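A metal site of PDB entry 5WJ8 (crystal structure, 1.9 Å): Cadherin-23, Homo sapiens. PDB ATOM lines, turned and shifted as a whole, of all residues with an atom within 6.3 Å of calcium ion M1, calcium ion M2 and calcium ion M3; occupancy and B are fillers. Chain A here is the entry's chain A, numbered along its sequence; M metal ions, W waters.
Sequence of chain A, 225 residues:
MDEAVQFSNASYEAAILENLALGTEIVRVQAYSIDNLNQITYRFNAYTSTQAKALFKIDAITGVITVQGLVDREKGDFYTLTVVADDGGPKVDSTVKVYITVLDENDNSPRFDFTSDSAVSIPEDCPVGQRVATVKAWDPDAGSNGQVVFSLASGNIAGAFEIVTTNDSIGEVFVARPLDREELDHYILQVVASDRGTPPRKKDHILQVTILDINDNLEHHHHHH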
ATOM      1  N   GLU A  18      -0.028 -11.888 -18.176  1.00  0.00           N
ATOM      2  CA  GLU A  18       0.454 -10.527 -17.887  1.00  0.00           C
ATOM      3  C   GLU A  18       1.844 -10.315 -18.501  1.00  0.00           C
ATOM      4  O   GLU A  18       2.540 -11.279 -18.814  1.00  0.00           O
ATOM      5  CB  GLU A  18       0.502 -10.249 -16.385  1.00  0.00           C
ATOM      6  CG  GLU A  18       1.351 -11.202 -15.549  1.00  0.00           C
ATOM      7  CD  GLU A  18       1.538 -10.698 -14.120  1.00  0.00           C
ATOM      8  OE1 GLU A  18       1.801 -11.515 -13.211  1.00  0.00           O
ATOM      9  OE2 GLU A  18       1.442  -9.466 -13.908  1.00  0.00           O
ATOM     10  N   ASN A  19       2.228  -9.053 -18.650  1.00  0.00           N
ATOM     11  CA  ASN A  19       3.554  -8.619 -19.140  1.00  0.00           C
ATOM     12  C   ASN A  19       3.807  -8.849 -20.650  1.00  0.00           C
ATOM     13  O   ASN A  19       4.921  -8.705 -21.126  1.00  0.00           O
ATOM     14  CB  ASN A  19       4.712  -9.220 -18.316  1.00  0.00           C
ATOM     15  CG  ASN A  19       4.636  -8.880 -16.830  1.00  0.00           C
ATOM     16  OD1 ASN A  19       4.289  -7.751 -16.443  1.00  0.00           O
ATOM     17  ND2 ASN A  19       4.963  -9.846 -15.982  1.00  0.00           N
ATOM     18  N   VAL A  71       0.317  -4.564 -19.055  1.00  0.00           N
ATOM     19  CA  VAL A  71      -0.696  -5.413 -18.453  1.00  0.00           C
ATOM     20  C   VAL A  71      -0.110  -6.115 -17.221  1.00  0.00           C
ATOM     21  O   VAL A  71       0.834  -6.934 -17.358  1.00  0.00           O
ATOM     22  CB  VAL A  71      -1.249  -6.457 -19.451  1.00  0.00           C
ATOM     23  CG1 VAL A  71      -2.235  -7.406 -18.787  1.00  0.00           C
ATOM     24  CG2 VAL A  71      -1.940  -5.755 -20.603  1.00  0.00           C
ATOM     25  N   ASP A  72      -0.639  -5.757 -16.036  1.00  0.00           N
ATOM     26  CA  ASP A  72      -0.094  -6.220 -14.759  1.00  0.00           C
ATOM     27  C   ASP A  72      -1.203  -6.887 -13.982  1.00  0.00           C
ATOM     28  O   ASP A  72      -2.139  -6.214 -13.539  1.00  0.00           O
ATOM     29  CB  ASP A  72       0.500  -5.037 -14.002  1.00  0.00           C
ATOM     30  CG  ASP A  72       1.121  -5.413 -12.664  1.00  0.00           C
ATOM     31  OD1 ASP A  72       1.150  -6.603 -12.282  1.00  0.00           O
ATOM     32  OD2 ASP A  72       1.559  -4.487 -11.972  1.00  0.00           O
ATOM     33  N   ARG A  73      -1.120  -8.207 -13.807  1.00  0.00           N
ATOM     34  CA  ARG A  73      -2.145  -8.939 -13.076  1.00  0.00           C
ATOM     35  C   ARG A  73      -2.276  -8.422 -11.634  1.00  0.00           C
ATOM     36  O   ARG A  73      -3.369  -8.414 -11.066  1.00  0.00           O
ATOM     37  CB  ARG A  73      -1.859 -10.447 -13.042  1.00  0.00           C
ATOM     38  CG  ARG A  73      -3.089 -11.270 -12.635  1.00  0.00           C
ATOM     39  CD  ARG A  73      -2.712 -12.486 -11.830  1.00  0.00           C
ATOM     40  NE  ARG A  73      -2.010 -12.082 -10.610  1.00  0.00           N
ATOM     41  CZ  ARG A  73      -2.583 -11.756  -9.446  1.00  0.00           C
ATOM     42  NH1 ARG A  73      -3.907 -11.839  -9.264  1.00  0.00           N
ATOM     43  NH2 ARG A  73      -1.809 -11.376  -8.439  1.00  0.00           N
ATOM     44  N   GLU A  74      -1.169  -7.959 -11.069  1.00  0.00           N
ATOM     45  CA  GLU A  74      -1.180  -7.404  -9.713  1.00  0.00           C
ATOM     46  C   GLU A  74      -2.014  -6.100  -9.594  1.00  0.00           C
ATOM     47  O   GLU A  74      -2.420  -5.727  -8.490  1.00  0.00           O
ATOM     48  CB  GLU A  74       0.250  -7.181  -9.223  1.00  0.00           C
ATOM     49  CG  GLU A  74       0.945  -8.441  -8.731  1.00  0.00           C
ATOM     50  CD  GLU A  74       1.188  -9.500  -9.813  1.00  0.00           C
ATOM     51  OE1 GLU A  74       1.887  -9.237 -10.824  1.00  0.00           O
ATOM     52  OE2 GLU A  74       0.687 -10.621  -9.653  1.00  0.00           O
ATOM     53  N   LYS A  75      -2.268  -5.412 -10.707  1.00  0.00           N
ATOM     54  CA  LYS A  75      -3.129  -4.209 -10.719  1.00  0.00           C
ATOM     55  C   LYS A  75      -4.554  -4.465 -11.208  1.00  0.00           C
ATOM     56  O   LYS A  75      -5.409  -3.627 -11.026  1.00  0.00           O
ATOM     57  CB  LYS A  75      -2.483  -3.127 -11.596  1.00  0.00           C
ATOM     58  CG  LYS A  75      -1.246  -2.508 -10.979  1.00  0.00           C
ATOM     59  CD  LYS A  75      -0.693  -1.388 -11.853  1.00  0.00           C
ATOM     60  CE  LYS A  75       0.617  -0.784 -11.345  1.00  0.00           C
ATOM     61  NZ  LYS A  75       0.908  -0.972  -9.893  1.00  0.00           N
ATOM     62  N   LEU A 103      -3.819 -13.687 -16.659  1.00  0.00           N
ATOM     63  CA  LEU A 103      -3.275 -14.810 -15.917  1.00  0.00           C
ATOM     64  C   LEU A 103      -1.952 -14.415 -15.286  1.00  0.00           C
ATOM     65  O   LEU A 103      -1.228 -13.566 -15.835  1.00  0.00           O
ATOM     66  CB  LEU A 103      -2.991 -15.981 -16.879  1.00  0.00           C
ATOM     67  CG  LEU A 103      -4.134 -16.467 -17.779  1.00  0.00           C
ATOM     68  CD1 LEU A 103      -3.686 -17.610 -18.686  1.00  0.00           C
ATOM     69  CD2 LEU A 103      -5.316 -16.934 -16.934  1.00  0.00           C
ATOM     70  N   ASP A 104      -1.620 -15.090 -14.192  1.00  0.00           N
ATOM     71  CA  ASP A 104      -0.454 -14.759 -13.385  1.00  0.00           C
ATOM     72  C   ASP A 104       0.853 -15.298 -13.946  1.00  0.00           C
ATOM     73  O   ASP A 104       0.905 -16.448 -14.383  1.00  0.00           O
ATOM     74  CB  ASP A 104      -0.618 -15.317 -11.966  1.00  0.00           C
ATOM     75  CG  ASP A 104       0.346 -14.684 -10.974  1.00  0.00           C
ATOM     76  OD1 ASP A 104       0.571 -13.460 -10.981  1.00  0.00           O
ATOM     77  OD2 ASP A 104       0.886 -15.415 -10.141  1.00  0.00           O
ATOM     78  N   GLU A 105       1.877 -14.454 -13.914  1.00  0.00           N
ATOM     79  CA  GLU A 105       3.280 -14.845 -14.023  1.00  0.00           C
ATOM     80  C   GLU A 105       3.941 -14.668 -12.687  1.00  0.00           C
ATOM     81  O   GLU A 105       3.575 -13.768 -11.898  1.00  0.00           O
ATOM     82  CB  GLU A 105       4.019 -13.983 -15.039  1.00  0.00           C
ATOM     83  CG  GLU A 105       3.655 -14.414 -16.456  1.00  0.00           C
ATOM     84  CD  GLU A 105       4.485 -13.744 -17.528  1.00  0.00           C
ATOM     85  OE1 GLU A 105       5.085 -12.663 -17.259  1.00  0.00           O
ATOM     86  OE2 GLU A 105       4.501 -14.317 -18.645  1.00  0.00           O
ATOM     87  N   ASN A 106       4.958 -15.489 -12.446  1.00  0.00           N
ATOM     88  CA  ASN A 106       5.744 -15.380 -11.227  1.00  0.00           C
ATOM     89  C   ASN A 106       6.778 -14.265 -11.400  1.00  0.00           C
ATOM     90  O   ASN A 106       7.989 -14.502 -11.460  1.00  0.00           O
ATOM     91  CB  ASN A 106       6.391 -16.709 -10.850  1.00  0.00           C
ATOM     92  CG  ASN A 106       6.832 -16.711  -9.404  1.00  0.00           C
ATOM     93  OD1 ASN A 106       6.331 -15.906  -8.631  1.00  0.00           O
ATOM     94  ND2 ASN A 106       7.771 -17.587  -9.023  1.00  0.00           N
ATOM     95  N   ASP A 107       6.292 -13.030 -11.428  1.00  0.00           N
ATOM     96  CA  ASP A 107       7.118 -11.901 -11.791  1.00  0.00           C
ATOM     97  C   ASP A 107       7.554 -11.090 -10.570  1.00  0.00           C
ATOM     98  O   ASP A 107       8.113 -10.020 -10.715  1.00  0.00           O
ATOM     99  CB  ASP A 107       6.478 -11.043 -12.898  1.00  0.00           C
ATOM    100  CG  ASP A 107       5.113 -10.441 -12.525  1.00  0.00           C
ATOM    101  OD1 ASP A 107       4.400 -10.898 -11.608  1.00  0.00           O
ATOM    102  OD2 ASP A 107       4.721  -9.513 -13.241  1.00  0.00           O
ATOM    103  N   ASN A 108       7.330 -11.646  -9.381  1.00  0.00           N
ATOM    104  CA  ASN A 108       7.828 -11.051  -8.149  1.00  0.00           C
ATOM    105  C   ASN A 108       8.525 -12.086  -7.293  1.00  0.00           C
ATOM    106  O   ASN A 108       8.048 -13.219  -7.147  1.00  0.00           O
ATOM    107  CB  ASN A 108       6.684 -10.401  -7.348  1.00  0.00           C
ATOM    108  CG  ASN A 108       6.024  -9.272  -8.101  1.00  0.00           C
ATOM    109  OD1 ASN A 108       6.424  -8.111  -7.970  1.00  0.00           O
ATOM    110  ND2 ASN A 108       5.046  -9.604  -8.928  1.00  0.00           N
ATOM    111  N   SER A 109       9.655 -11.677  -6.721  1.00  0.00           N
ATOM    112  CA  SER A 109      10.327 -12.409  -5.659  1.00  0.00           C
ATOM    113  C   SER A 109       9.795 -11.910  -4.319  1.00  0.00           C
ATOM    114  O   SER A 109       9.361 -10.768  -4.218  1.00  0.00           O
ATOM    115  CB  SER A 109      11.832 -12.134  -5.674  1.00  0.00           C
ATOM    116  OG  SER A 109      12.417 -12.557  -6.889  1.00  0.00           O
ATOM    117  N   PRO A 110       9.863 -12.758  -3.273  1.00  0.00           N
ATOM    118  CA  PRO A 110       9.584 -12.273  -1.920  1.00  0.00           C
ATOM    119  C   PRO A 110      10.447 -11.073  -1.587  1.00  0.00           C
ATOM    120  O   PRO A 110      11.616 -11.040  -1.944  1.00  0.00           O
ATOM    121  CB  PRO A 110       9.969 -13.474  -1.047  1.00  0.00           C
ATOM    122  CG  PRO A 110       9.720 -14.664  -1.915  1.00  0.00           C
ATOM    123  CD  PRO A 110      10.072 -14.216  -3.309  1.00  0.00           C
ATOM    124  N   ASP A 139       4.857 -11.318  -1.053  1.00  0.00           N
ATOM    125  CA  ASP A 139       4.929 -11.660  -2.462  1.00  0.00           C
ATOM    126  C   ASP A 139       3.518 -11.487  -3.031  1.00  0.00           C
ATOM    127  O   ASP A 139       2.637 -12.269  -2.697  1.00  0.00           O
ATOM    128  CB  ASP A 139       5.439 -13.072  -2.622  1.00  0.00           C
ATOM    129  CG  ASP A 139       5.793 -13.415  -4.061  1.00  0.00           C
ATOM    130  OD1 ASP A 139       5.025 -13.062  -4.988  1.00  0.00           O
ATOM    131  OD2 ASP A 139       6.848 -14.066  -4.256  1.00  0.00           O
ATOM    132  N   PRO A 140       3.325 -10.488  -3.921  1.00  0.00           N
ATOM    133  CA  PRO A 140       2.008 -10.157  -4.460  1.00  0.00           C
ATOM    134  C   PRO A 140       1.453 -11.057  -5.579  1.00  0.00           C
ATOM    135  O   PRO A 140       0.340 -10.810  -6.044  1.00  0.00           O
ATOM    136  CB  PRO A 140       2.225  -8.745  -5.011  1.00  0.00           C
ATOM    137  CG  PRO A 140       3.654  -8.751  -5.444  1.00  0.00           C
ATOM    138  CD  PRO A 140       4.354  -9.552  -4.414  1.00  0.00           C
ATOM    139  N   ASP A 141       2.187 -12.079  -6.020  1.00  0.00           N
ATOM    140  CA  ASP A 141       1.683 -12.967  -7.072  1.00  0.00           C
ATOM    141  C   ASP A 141       0.520 -13.838  -6.556  1.00  0.00           C
ATOM    142  O   ASP A 141       0.286 -13.933  -5.355  1.00  0.00           O
ATOM    143  CB  ASP A 141       2.810 -13.850  -7.636  1.00  0.00           C
ATOM    144  CG  ASP A 141       3.912 -13.035  -8.324  1.00  0.00           C
ATOM    145  OD1 ASP A 141       3.632 -12.109  -9.113  1.00  0.00           O
ATOM    146  OD2 ASP A 141       5.105 -13.347  -8.076  1.00  0.00           O
ATOM    147  N   ALA A 142      -0.186 -14.492  -7.470  1.00  0.00           N
ATOM    148  CA  ALA A 142      -1.325 -15.318  -7.143  1.00  0.00           C
ATOM    149  C   ALA A 142      -0.945 -16.750  -6.821  1.00  0.00           C
ATOM    150  O   ALA A 142       0.097 -17.234  -7.267  1.00  0.00           O
ATOM    151  CB  ALA A 142      -2.354 -15.284  -8.261  1.00  0.00           C
ATOM    152  N   SER A 144       0.197 -20.292  -5.622  1.00  0.00           N
ATOM    153  CA  SER A 144       1.557 -20.741  -5.276  1.00  0.00           C
ATOM    154  C   SER A 144       2.658 -19.711  -5.527  1.00  0.00           C
ATOM    155  O   SER A 144       3.603 -19.608  -4.724  1.00  0.00           O
ATOM    156  CB  SER A 144       1.903 -22.007  -6.050  1.00  0.00           C
ATOM    157  OG  SER A 144       1.085 -23.076  -5.621  1.00  0.00           O
ATOM    158  N   ASN A 145       2.564 -18.951  -6.611  1.00  0.00           N
ATOM    159  CA  ASN A 145       3.566 -17.937  -6.967  1.00  0.00           C
ATOM    160  C   ASN A 145       3.767 -16.872  -5.891  1.00  0.00           C
ATOM    161  O   ASN A 145       4.846 -16.236  -5.868  1.00  0.00           O
ATOM    162  CB  ASN A 145       3.217 -17.211  -8.278  1.00  0.00           C
ATOM    163  CG  ASN A 145       3.387 -18.080  -9.514  1.00  0.00           C
ATOM    164  OD1 ASN A 145       4.100 -19.077  -9.501  1.00  0.00           O
ATOM    165  ND2 ASN A 145       2.751 -17.652 -10.604  1.00  0.00           N
ATOM    166  N   GLY A 146       2.741 -16.645  -5.088  1.00  0.00           N
ATOM    167  CA  GLY A 146       2.752 -15.638  -4.034  1.00  0.00           C
ATOM    168  C   GLY A 146       2.792 -16.170  -2.615  1.00  0.00           C
ATOM    169  O   GLY A 146       2.781 -15.395  -1.672  1.00  0.00           O
ATOM    170  N   GLN A 147       2.824 -17.487  -2.445  1.00  0.00           N
ATOM    171  CA  GLN A 147       3.006 -18.114  -1.125  1.00  0.00           C
ATOM    172  C   GLN A 147       4.468 -18.142  -0.732  1.00  0.00           C
ATOM    173  O   GLN A 147       5.273 -18.608  -1.514  1.00  0.00           O
ATOM    174  CB  GLN A 147       2.495 -19.553  -1.154  1.00  0.00           C
ATOM    175  CG  GLN A 147       0.986 -19.596  -1.237  1.00  0.00           C
ATOM    176  CD  GLN A 147       0.429 -20.993  -1.354  1.00  0.00           C
ATOM    177  OE1 GLN A 147       1.093 -21.923  -1.829  1.00  0.00           O
ATOM    178  NE2 GLN A 147      -0.817 -21.141  -0.947  1.00  0.00           N
ATOM    179  N   ASP A 195       9.261 -18.215  -2.717  1.00  0.00           N
ATOM    180  CA  ASP A 195       7.871 -18.453  -3.107  1.00  0.00           C
ATOM    181  C   ASP A 195       7.722 -19.925  -3.506  1.00  0.00           C
ATOM    182  O   ASP A 195       8.697 -20.684  -3.469  1.00  0.00           O
ATOM    183  CB  ASP A 195       7.330 -17.471  -4.152  1.00  0.00           C
ATOM    184  CG  ASP A 195       7.993 -17.579  -5.515  1.00  0.00           C
ATOM    185  OD1 ASP A 195       8.445 -18.689  -5.903  1.00  0.00           O
ATOM    186  OD2 ASP A 195       8.061 -16.531  -6.210  1.00  0.00           O
ATOM    187  N   ARG A 196       6.519 -20.350  -3.874  1.00  0.00           N
ATOM    188  CA  ARG A 196       6.297 -21.693  -4.368  1.00  0.00           C
ATOM    189  C   ARG A 196       5.986 -21.725  -5.856  1.00  0.00           C
ATOM    190  O   ARG A 196       5.235 -22.565  -6.302  1.00  0.00           O
ATOM    191  CB  ARG A 196       5.161 -22.362  -3.623  1.00  0.00           C
ATOM    192  CG  ARG A 196       5.355 -22.452  -2.133  1.00  0.00           C
ATOM    193  CD  ARG A 196       4.183 -23.207  -1.533  1.00  0.00           C
ATOM    194  NE  ARG A 196       4.636 -24.090  -0.473  1.00  0.00           N
ATOM    195  CZ  ARG A 196       4.523 -23.869   0.844  1.00  0.00           C
ATOM    196  NH1 ARG A 196       3.938 -22.761   1.327  1.00  0.00           N
ATOM    197  NH2 ARG A 196       5.019 -24.766   1.681  1.00  0.00           N
ATOM    198  N   GLY A 197       6.584 -20.822  -6.627  1.00  0.00           N
ATOM    199  CA  GLY A 197       6.549 -20.929  -8.083  1.00  0.00           C
ATOM    200  C   GLY A 197       7.376 -22.118  -8.561  1.00  0.00           C
ATOM    201  O   GLY A 197       8.095 -22.735  -7.782  1.00  0.00           O
ATOM    202  N   ARG A 201      11.239 -18.491  -6.721  1.00  0.00           N
ATOM    203  CA  ARG A 201      12.035 -17.280  -6.637  1.00  0.00           C
ATOM    204  C   ARG A 201      12.326 -17.073  -5.172  1.00  0.00           C
ATOM    205  O   ARG A 201      11.483 -17.372  -4.313  1.00  0.00           O
ATOM    206  CB  ARG A 201      11.270 -16.093  -7.192  1.00  0.00           C
ATOM    207  CG  ARG A 201      10.975 -16.269  -8.675  1.00  0.00           C
ATOM    208  CD  ARG A 201      10.276 -15.102  -9.333  1.00  0.00           C
ATOM    209  NE  ARG A 201      11.012 -13.839  -9.216  1.00  0.00           N
ATOM    210  CZ  ARG A 201      10.984 -12.849 -10.091  1.00  0.00           C
ATOM    211  NH1 ARG A 201      10.231 -12.892 -11.195  1.00  0.00           N
ATOM    212  NH2 ARG A 201      11.729 -11.771  -9.856  1.00  0.00           N
HETATM  213 CA    CA M   1       6.411 -14.685  -6.569  1.00  0.00          CA
HETATM  214 CA    CA M   2       2.331 -11.856 -11.050  1.00  0.00          CA
HETATM  215 CA    CA M   3       2.858  -8.193 -12.445  1.00  0.00          CA
HETATM  216  O   HOH W   1       3.549  -6.765 -14.144  1.00  0.00           O
HETATM  217  O   HOH W   2       4.287  -7.354 -10.828  1.00  0.00           O
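The side-chain carboxylate of Glu 18 sits close to the backbone NH of Arg 73. The backbone NH of Glu 18 sits at hydrogen-bond distance from the backbone carbonyl oxygen of Leu 103, at 3.1 Å. ND2 of Asn 108 sits close to OD1 of Asp 107 (3.0 Å). The side-chain carboxylate (OD2) of Asp 107 sits close to the side-chain amide nitrogen (ND2) of Asn 19 (2.8 Å). The guanidinium group (NE) of Arg 73 sits close to the side-chain carboxylate (OD1) of Asp 104, 2.9 Å away. The backbone carbonyl oxygen (O) of Asn 106 is in hydrogen-bond range of the guanidinium group (NH1) of Arg 201 (2.8 Å). OE1 of Glu 105 sits at hydrogen-bond distance from ND2 of Asn 19, 3.1 Å away. O of Arg 201 is in hydrogen-bond range of N of Asp 195, at 2.9 Å.
Within 4 Å of calcium ion M1: Asn 106, Asn 108, Asp 139, Asp 141, Asn 145 and Asp 195. Along chain A the residues within 4 Å of calcium ion M1 span positions 106 to 195.
Within 4 Å of calcium ion M2: Glu 18, Glu 74, Asp 104, Glu 105, Asp 107 and Asp 141. The nearest printed residue that does not touch calcium ion M2 is Asn 108 (4.1 Å).
Calcium ion M1 is bound by the backbone carbonyl oxygen (O) of Asn 108 (2.3 Å), the backbone carbonyl oxygen (O) of Asn 145 (2.3 Å), the side-chain amide oxygen (OD1) of Asn 106 (2.4 Å), the side-chain carboxylate (OD2) of Asp 141 (2.4 Å), the side-chain carboxylate (OD2) of Asp 139 (2.4 Å), the side-chain carboxylate (OD2) of Asp 195 (2.5 Å) and the side-chain carboxylate (OD1) of Asp 139 (2.7 Å).
Calcium ion M2 is bound by the side-chain carboxylate (OE1) of Glu 18 (2.3 Å), the side-chain carboxylate (OD1) of Asp 107 (2.3 Å), the side-chain carboxylate (OD1) of Asp 141 (2.3 Å), the side-chain carboxylate (OD1) of Asp 104 (2.4 Å), the backbone carbonyl oxygen (O) of Glu 105 (2.4 Å), the side-chain carboxylate (OE2) of Glu 74 (2.5 Å) and the side-chain carboxylate (OE1) of Glu 74 (2.7 Å).
Calcium ion M3 is bound by OE1 of Glu 74 (2.2 Å). Calcium ion M3 is bound by water W2, at 2.3 Å. Water W1 is bound to calcium ion M3, at 2.3 Å. The side-chain carboxylate (OD1) of Asp 72 binds calcium ion M3, 2.3 Å away. Calcium ion M3 is bound by OE2 of Glu 18. OD2 of Asp 107 binds calcium ion M3.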
